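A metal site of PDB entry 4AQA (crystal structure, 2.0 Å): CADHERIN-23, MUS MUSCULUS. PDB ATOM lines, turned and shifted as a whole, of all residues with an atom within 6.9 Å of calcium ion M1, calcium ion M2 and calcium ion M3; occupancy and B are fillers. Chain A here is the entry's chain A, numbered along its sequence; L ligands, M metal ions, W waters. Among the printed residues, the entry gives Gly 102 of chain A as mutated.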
ATOM      1  N   GLU A  22     -26.816  -6.221  29.534  1.00  0.00           N
ATOM      2  CA  GLU A  22     -27.396  -7.454  30.054  1.00  0.00           C
ATOM      3  C   GLU A  22     -27.278  -7.551  31.572  1.00  0.00           C
ATOM      4  O   GLU A  22     -27.951  -8.386  32.184  1.00  0.00           O
ATOM      5  CB  GLU A  22     -26.776  -8.688  29.408  1.00  0.00           C
ATOM      6  CG  GLU A  22     -25.304  -8.961  29.769  1.00  0.00           C
ATOM      7  CD  GLU A  22     -24.816 -10.314  29.290  1.00  0.00           C
ATOM      8  OE1 GLU A  22     -25.624 -11.263  29.237  1.00  0.00           O
ATOM      9  OE2 GLU A  22     -23.599 -10.457  28.991  1.00  0.00           O
ATOM     10  N   LEU A  71     -32.146  -9.667  31.055  1.00  0.00           N
ATOM     11  CA  LEU A  71     -31.678  -9.914  29.695  1.00  0.00           C
ATOM     12  C   LEU A  71     -30.472 -10.819  29.750  1.00  0.00           C
ATOM     13  O   LEU A  71     -29.841 -10.997  30.801  1.00  0.00           O
ATOM     14  CB  LEU A  71     -31.310  -8.606  28.993  1.00  0.00           C
ATOM     15  CG  LEU A  71     -32.424  -7.568  28.947  1.00  0.00           C
ATOM     16  CD1 LEU A  71     -31.882  -6.280  28.352  1.00  0.00           C
ATOM     17  CD2 LEU A  71     -33.617  -8.092  28.158  1.00  0.00           C
ATOM     18  N   ASP A  72     -30.154 -11.428  28.620  1.00  0.00           N
ATOM     19  CA  ASP A  72     -29.009 -12.292  28.517  1.00  0.00           C
ATOM     20  C   ASP A  72     -28.465 -12.237  27.105  1.00  0.00           C
ATOM     21  O   ASP A  72     -29.053 -12.814  26.190  1.00  0.00           O
ATOM     22  CB  ASP A  72     -29.386 -13.723  28.890  1.00  0.00           C
ATOM     23  CG  ASP A  72     -28.220 -14.664  28.826  1.00  0.00           C
ATOM     24  OD1 ASP A  72     -27.078 -14.206  28.497  1.00  0.00           O
ATOM     25  OD2 ASP A  72     -28.418 -15.872  29.098  1.00  0.00           O
ATOM     26  N   ARG A  73     -27.327 -11.565  26.926  1.00  0.00           N
ATOM     27  CA  ARG A  73     -26.737 -11.399  25.613  1.00  0.00           C
ATOM     28  C   ARG A  73     -26.384 -12.739  24.961  1.00  0.00           C
ATOM     29  O   ARG A  73     -26.455 -12.885  23.736  1.00  0.00           O
ATOM     30  CB  ARG A  73     -25.495 -10.523  25.699  1.00  0.00           C
ATOM     31  CG  ARG A  73     -24.988 -10.107  24.340  1.00  0.00           C
ATOM     32  CD  ARG A  73     -23.478 -10.029  24.320  1.00  0.00           C
ATOM     33  NE  ARG A  73     -22.881 -11.338  24.481  1.00  0.00           N
ATOM     34  CZ  ARG A  73     -22.676 -12.211  23.495  1.00  0.00           C
ATOM     35  NH1 ARG A  73     -23.079 -11.940  22.248  1.00  0.00           N
ATOM     36  NH2 ARG A  73     -22.110 -13.370  23.764  1.00  0.00           N
ATOM     37  N   GLU A  74     -26.011 -13.718  25.780  1.00  0.00           N
ATOM     38  CA  GLU A  74     -25.647 -15.030  25.262  1.00  0.00           C
ATOM     39  C   GLU A  74     -26.835 -15.740  24.637  1.00  0.00           C
ATOM     40  O   GLU A  74     -26.649 -16.551  23.740  1.00  0.00           O
ATOM     41  CB  GLU A  74     -24.987 -15.907  26.338  1.00  0.00           C
ATOM     42  CG  GLU A  74     -23.511 -15.598  26.593  1.00  0.00           C
ATOM     43  CD  GLU A  74     -23.284 -14.199  27.180  1.00  0.00           C
ATOM     44  OE1 GLU A  74     -23.965 -13.838  28.171  1.00  0.00           O
ATOM     45  OE2 GLU A  74     -22.395 -13.469  26.633  1.00  0.00           O
ATOM     46  N   THR A  75     -28.044 -15.434  25.102  1.00  0.00           N
ATOM     47  CA  THR A  75     -29.265 -16.010  24.532  1.00  0.00           C
ATOM     48  C   THR A  75     -29.799 -15.184  23.361  1.00  0.00           C
ATOM     49  O   THR A  75     -30.206 -15.741  22.353  1.00  0.00           O
ATOM     50  CB  THR A  75     -30.375 -16.100  25.578  1.00  0.00           C
ATOM     51  OG1 THR A  75     -29.915 -16.869  26.692  1.00  0.00           O
ATOM     52  CG2 THR A  75     -31.611 -16.780  24.973  1.00  0.00           C
ATOM     53  N   GLY A 101     -26.319  -5.239  25.545  1.00  0.00           N
ATOM     54  CA  GLY A 101     -24.902  -5.046  25.820  1.00  0.00           C
ATOM     55  C   GLY A 101     -24.320  -6.176  26.649  1.00  0.00           C
ATOM     56  O   GLY A 101     -25.007  -6.714  27.524  1.00  0.00           O
ATOM     57  N   GLY A 102     -23.062  -6.515  26.385  1.00  0.00           N
ATOM     58  CA  GLY A 102     -22.409  -7.654  26.973  1.00  0.00           C
ATOM     59  C   GLY A 102     -21.638  -7.273  28.203  1.00  0.00           C
ATOM     60  O   GLY A 102     -21.151  -6.163  28.324  1.00  0.00           O
ATOM     61  N   VAL A 103     -21.610  -8.187  29.176  1.00  0.00           N
ATOM     62  CA  VAL A 103     -20.632  -8.108  30.254  1.00  0.00           C
ATOM     63  C   VAL A 103     -20.139  -9.530  30.464  1.00  0.00           C
ATOM     64  O   VAL A 103     -20.769 -10.484  30.054  1.00  0.00           O
ATOM     65  CB  VAL A 103     -21.241  -7.606  31.581  1.00  0.00           C
ATOM     66  CG1 VAL A 103     -21.982  -6.279  31.410  1.00  0.00           C
ATOM     67  CG2 VAL A 103     -22.159  -8.667  32.184  1.00  0.00           C
ATOM     68  N   ASN A 104     -18.997  -9.679  31.116  1.00  0.00           N
ATOM     69  CA  ASN A 104     -18.454 -10.999  31.368  1.00  0.00           C
ATOM     70  C   ASN A 104     -19.259 -11.674  32.478  1.00  0.00           C
ATOM     71  O   ASN A 104     -19.133 -11.299  33.656  1.00  0.00           O
ATOM     72  CB  ASN A 104     -16.989 -10.909  31.759  1.00  0.00           C
ATOM     73  CG  ASN A 104     -16.328 -12.278  31.784  1.00  0.00           C
ATOM     74  OD1 ASN A 104     -16.471 -13.058  30.840  1.00  0.00           O
ATOM     75  ND2 ASN A 104     -15.627 -12.585  32.873  1.00  0.00           N
ATOM     76  N   ASP A 105     -20.105 -12.632  32.104  1.00  0.00           N
ATOM     77  CA  ASP A 105     -20.861 -13.373  33.118  1.00  0.00           C
ATOM     78  C   ASP A 105     -20.859 -14.889  32.996  1.00  0.00           C
ATOM     79  O   ASP A 105     -21.625 -15.567  33.674  1.00  0.00           O
ATOM     80  CB  ASP A 105     -22.284 -12.796  33.283  1.00  0.00           C
ATOM     81  CG  ASP A 105     -23.134 -12.833  32.010  1.00  0.00           C
ATOM     82  OD1 ASP A 105     -22.633 -13.118  30.891  1.00  0.00           O
ATOM     83  OD2 ASP A 105     -24.357 -12.546  32.128  1.00  0.00           O
ATOM     84  N   ASN A 106     -19.965 -15.452  32.186  1.00  0.00           N
ATOM     85  CA  ASN A 106     -19.749 -16.902  32.172  1.00  0.00           C
ATOM     86  C   ASN A 106     -18.289 -17.254  32.414  1.00  0.00           C
ATOM     87  O   ASN A 106     -17.401 -16.489  32.045  1.00  0.00           O
ATOM     88  CB  ASN A 106     -20.166 -17.519  30.836  1.00  0.00           C
ATOM     89  CG  ASN A 106     -21.624 -17.260  30.502  1.00  0.00           C
ATOM     90  OD1 ASN A 106     -22.459 -18.155  30.685  1.00  0.00           O
ATOM     91  ND2 ASN A 106     -21.957 -16.049  30.032  1.00  0.00           N
ATOM     92  N   ALA A 107     -18.064 -18.408  33.041  1.00  0.00           N
ATOM     93  CA  ALA A 107     -16.722 -18.932  33.172  1.00  0.00           C
ATOM     94  C   ALA A 107     -16.562 -19.886  32.012  1.00  0.00           C
ATOM     95  O   ALA A 107     -17.562 -20.259  31.427  1.00  0.00           O
ATOM     96  CB  ALA A 107     -16.556 -19.666  34.499  1.00  0.00           C
ATOM     97  N   PRO A 108     -15.324 -20.246  31.658  1.00  0.00           N
ATOM     98  CA  PRO A 108     -15.120 -21.273  30.629  1.00  0.00           C
ATOM     99  C   PRO A 108     -15.647 -22.656  31.006  1.00  0.00           C
ATOM    100  O   PRO A 108     -15.806 -22.964  32.187  1.00  0.00           O
ATOM    101  CB  PRO A 108     -13.602 -21.311  30.445  1.00  0.00           C
ATOM    102  CG  PRO A 108     -13.103 -20.023  31.006  1.00  0.00           C
ATOM    103  CD  PRO A 108     -14.038 -19.693  32.127  1.00  0.00           C
ATOM    104  N   ASP A 136     -15.778 -20.367  26.038  1.00  0.00           N
ATOM    105  CA  ASP A 136     -16.440 -19.356  26.884  1.00  0.00           C
ATOM    106  C   ASP A 136     -17.244 -18.474  25.950  1.00  0.00           C
ATOM    107  O   ASP A 136     -16.664 -17.926  25.038  1.00  0.00           O
ATOM    108  CB  ASP A 136     -15.376 -18.537  27.597  1.00  0.00           C
ATOM    109  CG  ASP A 136     -15.966 -17.560  28.609  1.00  0.00           C
ATOM    110  OD1 ASP A 136     -17.016 -16.903  28.325  1.00  0.00           O
ATOM    111  OD2 ASP A 136     -15.356 -17.445  29.706  1.00  0.00           O
ATOM    112  N   PRO A 137     -18.564 -18.330  26.181  1.00  0.00           N
ATOM    113  CA  PRO A 137     -19.465 -17.650  25.241  1.00  0.00           C
ATOM    114  C   PRO A 137     -19.534 -16.097  25.336  1.00  0.00           C
ATOM    115  O   PRO A 137     -20.179 -15.475  24.506  1.00  0.00           O
ATOM    116  CB  PRO A 137     -20.813 -18.258  25.595  1.00  0.00           C
ATOM    117  CG  PRO A 137     -20.712 -18.440  27.076  1.00  0.00           C
ATOM    118  CD  PRO A 137     -19.304 -18.897  27.317  1.00  0.00           C
ATOM    119  N   ASP A 138     -18.866 -15.501  26.312  1.00  0.00           N
ATOM    120  CA  ASP A 138     -18.891 -14.044  26.453  1.00  0.00           C
ATOM    121  C   ASP A 138     -18.097 -13.383  25.327  1.00  0.00           C
ATOM    122  O   ASP A 138     -17.249 -14.014  24.707  1.00  0.00           O
ATOM    123  CB  ASP A 138     -18.327 -13.591  27.801  1.00  0.00           C
ATOM    124  CG  ASP A 138     -19.117 -14.131  28.998  1.00  0.00           C
ATOM    125  OD1 ASP A 138     -20.348 -13.833  29.118  1.00  0.00           O
ATOM    126  OD2 ASP A 138     -18.485 -14.825  29.819  1.00  0.00           O
ATOM    127  N   LEU A 139     -18.393 -12.111  25.085  1.00  0.00           N
ATOM    128  CA  LEU A 139     -17.736 -11.355  24.030  1.00  0.00           C
ATOM    129  C   LEU A 139     -16.292 -11.012  24.407  1.00  0.00           C
ATOM    130  O   LEU A 139     -15.974 -10.761  25.584  1.00  0.00           O
ATOM    131  CB  LEU A 139     -18.493 -10.068  23.721  1.00  0.00           C
ATOM    132  CG  LEU A 139     -19.823 -10.162  22.978  1.00  0.00           C
ATOM    133  CD1 LEU A 139     -20.316  -8.764  22.683  1.00  0.00           C
ATOM    134  CD2 LEU A 139     -19.696 -10.948  21.679  1.00  0.00           C
ATOM    135  N   ALA A 141     -12.577 -10.171  25.328  1.00  0.00           N
ATOM    136  CA  ALA A 141     -11.608 -10.642  26.305  1.00  0.00           C
ATOM    137  C   ALA A 141     -12.261 -11.632  27.251  1.00  0.00           C
ATOM    138  O   ALA A 141     -11.647 -12.605  27.687  1.00  0.00           O
ATOM    139  CB  ALA A 141     -10.986  -9.478  27.075  1.00  0.00           C
ATOM    140  N   GLY A 142     -13.527 -11.377  27.569  1.00  0.00           N
ATOM    141  CA  GLY A 142     -14.266 -12.266  28.435  1.00  0.00           C
ATOM    142  C   GLY A 142     -14.540 -13.620  27.817  1.00  0.00           C
ATOM    143  O   GLY A 142     -15.014 -14.486  28.510  1.00  0.00           O
ATOM    144  N   GLY A 143     -14.254 -13.800  26.531  1.00  0.00           N
ATOM    145  CA  GLY A 143     -14.478 -15.065  25.862  1.00  0.00           C
ATOM    146  C   GLY A 143     -13.218 -15.751  25.387  1.00  0.00           C
ATOM    147  O   GLY A 143     -13.297 -16.811  24.756  1.00  0.00           O
ATOM    148  N   SER A 144     -12.047 -15.166  25.671  1.00  0.00           N
ATOM    149  CA  SER A 144     -10.778 -15.666  25.176  1.00  0.00           C
ATOM    150  C   SER A 144     -10.071 -16.369  26.326  1.00  0.00           C
ATOM    151  O   SER A 144      -9.835 -15.775  27.382  1.00  0.00           O
ATOM    152  CB  SER A 144      -9.945 -14.507  24.611  1.00  0.00           C
ATOM    153  OG  SER A 144      -8.640 -14.938  24.208  1.00  0.00           O
ATOM    154  N   THR A 186      -9.112 -19.745  32.345  1.00  0.00           N
ATOM    155  CA  THR A 186      -9.653 -18.429  32.704  1.00  0.00           C
ATOM    156  C   THR A 186      -9.912 -17.607  31.459  1.00  0.00           C
ATOM    157  O   THR A 186      -9.174 -17.707  30.447  1.00  0.00           O
ATOM    158  CB  THR A 186      -8.739 -17.609  33.665  1.00  0.00           C
ATOM    159  OG1 THR A 186      -9.364 -16.346  33.977  1.00  0.00           O
ATOM    160  CG2 THR A 186      -7.387 -17.287  33.051  1.00  0.00           C
ATOM    161  N   ASP A 187     -10.962 -16.811  31.515  1.00  0.00           N
ATOM    162  CA  ASP A 187     -11.112 -15.749  30.521  1.00  0.00           C
ATOM    163  C   ASP A 187     -10.213 -14.581  30.915  1.00  0.00           C
ATOM    164  O   ASP A 187      -9.493 -14.641  31.923  1.00  0.00           O
ATOM    165  CB  ASP A 187     -12.574 -15.369  30.269  1.00  0.00           C
ATOM    166  CG  ASP A 187     -13.273 -14.795  31.513  1.00  0.00           C
ATOM    167  OD1 ASP A 187     -12.631 -14.038  32.252  1.00  0.00           O
ATOM    168  OD2 ASP A 187     -14.472 -15.124  31.703  1.00  0.00           O
ATOM    169  N   GLN A 188     -10.188 -13.566  30.062  1.00  0.00           N
ATOM    170  CA  GLN A 188      -9.308 -12.433  30.223  1.00  0.00           C
ATOM    171  C   GLN A 188     -10.062 -11.120  30.449  1.00  0.00           C
ATOM    172  O   GLN A 188      -9.544 -10.077  30.150  1.00  0.00           O
ATOM    173  CB  GLN A 188      -8.439 -12.313  28.975  1.00  0.00           C
ATOM    174  CG  GLN A 188      -7.447 -13.441  28.855  1.00  0.00           C
ATOM    175  CD  GLN A 188      -6.605 -13.346  27.623  1.00  0.00           C
ATOM    176  OE1 GLN A 188      -5.535 -12.732  27.637  1.00  0.00           O
ATOM    177  NE2 GLN A 188      -7.072 -13.957  26.534  1.00  0.00           N
ATOM    178  N   ASP A 189     -11.270 -11.170  30.982  1.00  0.00           N
ATOM    179  CA  ASP A 189     -11.963  -9.928  31.275  1.00  0.00           C
ATOM    180  C   ASP A 189     -11.078  -9.089  32.217  1.00  0.00           C
ATOM    181  O   ASP A 189     -10.424  -9.636  33.104  1.00  0.00           O
ATOM    182  CB  ASP A 189     -13.308 -10.211  31.937  1.00  0.00           C
ATOM    183  CG  ASP A 189     -14.135  -8.965  32.064  1.00  0.00           C
ATOM    184  OD1 ASP A 189     -14.508  -8.369  31.024  1.00  0.00           O
ATOM    185  OD2 ASP A 189     -14.436  -8.576  33.205  1.00  0.00           O
ATOM    186  N   ARG A 192     -13.501  -8.418  35.907  1.00  0.00           N
ATOM    187  CA  ARG A 192     -14.089  -9.584  36.565  1.00  0.00           C
ATOM    188  C   ARG A 192     -13.756 -10.876  35.807  1.00  0.00           C
ATOM    189  O   ARG A 192     -14.644 -11.487  35.211  1.00  0.00           O
ATOM    190  CB  ARG A 192     -15.611  -9.424  36.688  1.00  0.00           C
ATOM    191  CG  ARG A 192     -16.031  -8.219  37.517  1.00  0.00           C
ATOM    192  CD  ARG A 192     -17.542  -8.033  37.647  1.00  0.00           C
ATOM    193  NE  ARG A 192     -18.147  -9.216  38.252  1.00  0.00           N
ATOM    194  CZ  ARG A 192     -18.736 -10.218  37.589  1.00  0.00           C
ATOM    195  NH1 ARG A 192     -18.855 -10.212  36.273  1.00  0.00           N
ATOM    196  NH2 ARG A 192     -19.198 -11.258  38.280  1.00  0.00           N
ATOM    197  N   PRO A 193     -12.483 -11.293  35.815  1.00  0.00           N
ATOM    198  CA  PRO A 193     -12.166 -12.541  35.122  1.00  0.00           C
ATOM    199  C   PRO A 193     -12.797 -13.737  35.838  1.00  0.00           C
ATOM    200  O   PRO A 193     -12.952 -13.737  37.082  1.00  0.00           O
ATOM    201  CB  PRO A 193     -10.649 -12.615  35.174  1.00  0.00           C
ATOM    202  CG  PRO A 193     -10.301 -11.839  36.398  1.00  0.00           C
ATOM    203  CD  PRO A 193     -11.288 -10.710  36.453  1.00  0.00           C
ATOM    204  N   LEU A 194     -13.187 -14.732  35.043  1.00  0.00           N
ATOM    205  CA  LEU A 194     -13.846 -15.898  35.562  1.00  0.00           C
ATOM    206  C   LEU A 194     -13.094 -17.129  35.088  1.00  0.00           C
ATOM    207  O   LEU A 194     -12.540 -17.128  33.980  1.00  0.00           O
ATOM    208  CB  LEU A 194     -15.307 -15.927  35.123  1.00  0.00           C
ATOM    209  CG  LEU A 194     -16.220 -14.845  35.718  1.00  0.00           C
ATOM    210  CD1 LEU A 194     -17.611 -14.908  35.097  1.00  0.00           C
ATOM    211  CD2 LEU A 194     -16.311 -14.983  37.226  1.00  0.00           C
HETATM  212 CL1  LIG L   1     -20.570 -10.601  26.881  1.00  0.00          CL
HETATM  213 CA    CA M   1     -21.961 -12.106  28.805  1.00  0.00          CA
HETATM  214 CA    CA M   2     -16.293 -15.395  30.281  1.00  0.00          CA
HETATM  215 CA    CA M   3     -25.255 -13.426  30.117  1.00  0.00          CA
HETATM  216  O   HOH W   1     -27.161 -13.398  31.622  1.00  0.00           O
HETATM  217  O   HOH W   2     -24.867 -15.542  30.807  1.00  0.00           O
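The nearest printed residue that does not touch calcium ion M1 is Asn 106 (4.1 Å).
Six residues have an atom within 4 Å of calcium ion M2: Asn 104, Asn 106, Asp 136, Asp 138, Gly 142 and Asp 187. The nearest printed residue that does not touch calcium ion M2 is Ala 107 (4.5 Å).
Calcium ion M1 is bound by OE2 of Glu 22 (2.3 Å), O of Val 103 (2.4 Å), OD1 of Asp 138 (2.4 Å), OD1 of Asp 105 (2.4 Å), OE2 of Glu 74 (2.6 Å), OE1 of Glu 74 (2.7 Å) and CL1 of the ligand (2.8 Å).
Within 4 Å of calcium ion M3: Glu 22, Asp 72, Glu 74 and Asp 105.
Calcium ion M2 is bound by OD2 of Asp 138, OD2 of Asp 136, OD2 of Asp 187, O of Asn 106, O of Gly 142, OD1 of Asn 104 and OD1 of Asp 136.
Calcium ion M3 is bound by water W2 (2.3 Å), the side-chain carboxylate (OE1) of Glu 22 (2.4 Å), the side-chain carboxylate (OE1) of Glu 74 (2.4 Å), the side-chain carboxylate (OD2) of Asp 105 (2.4 Å), water W1 (2.4 Å), the side-chain carboxylate (OD1) of Asp 72 (2.6 Å) and the side-chain carboxylate (OD1) of Asp 105 (2.8 Å).
OE2 of Glu 74 sits close to NH2 of Arg 73, 2.9 Å away. The backbone carbonyl oxygen (O) of Arg 192 lies within hydrogen-bond range of the side-chain amide nitrogen (ND2) of Asn 104, at 2.8 Å. The backbone NH of Glu 22 is in hydrogen-bond range of the backbone carbonyl oxygen of Gly 101 (2.7 Å). N of Leu 194 lies within hydrogen-bond range of OD1 of Asp 187 (2.9 Å). OD2 of Asp 72 is in hydrogen-bond range of OG1 of Thr 75. The side-chain carboxylate (OE1) of Glu 22 sits close to the backbone NH (N) of Arg 73 (2.9 Å). The side-chain carboxylate (OD1) of Asp 187 sits at hydrogen-bond distance from the backbone NH (N) of Asp 189, 3.4 Å away. The side-chain amide nitrogen (ND2) of Asn 106 lies close to the side-chain carboxylate (OD1) of Asp 105, 3.1 Å away.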
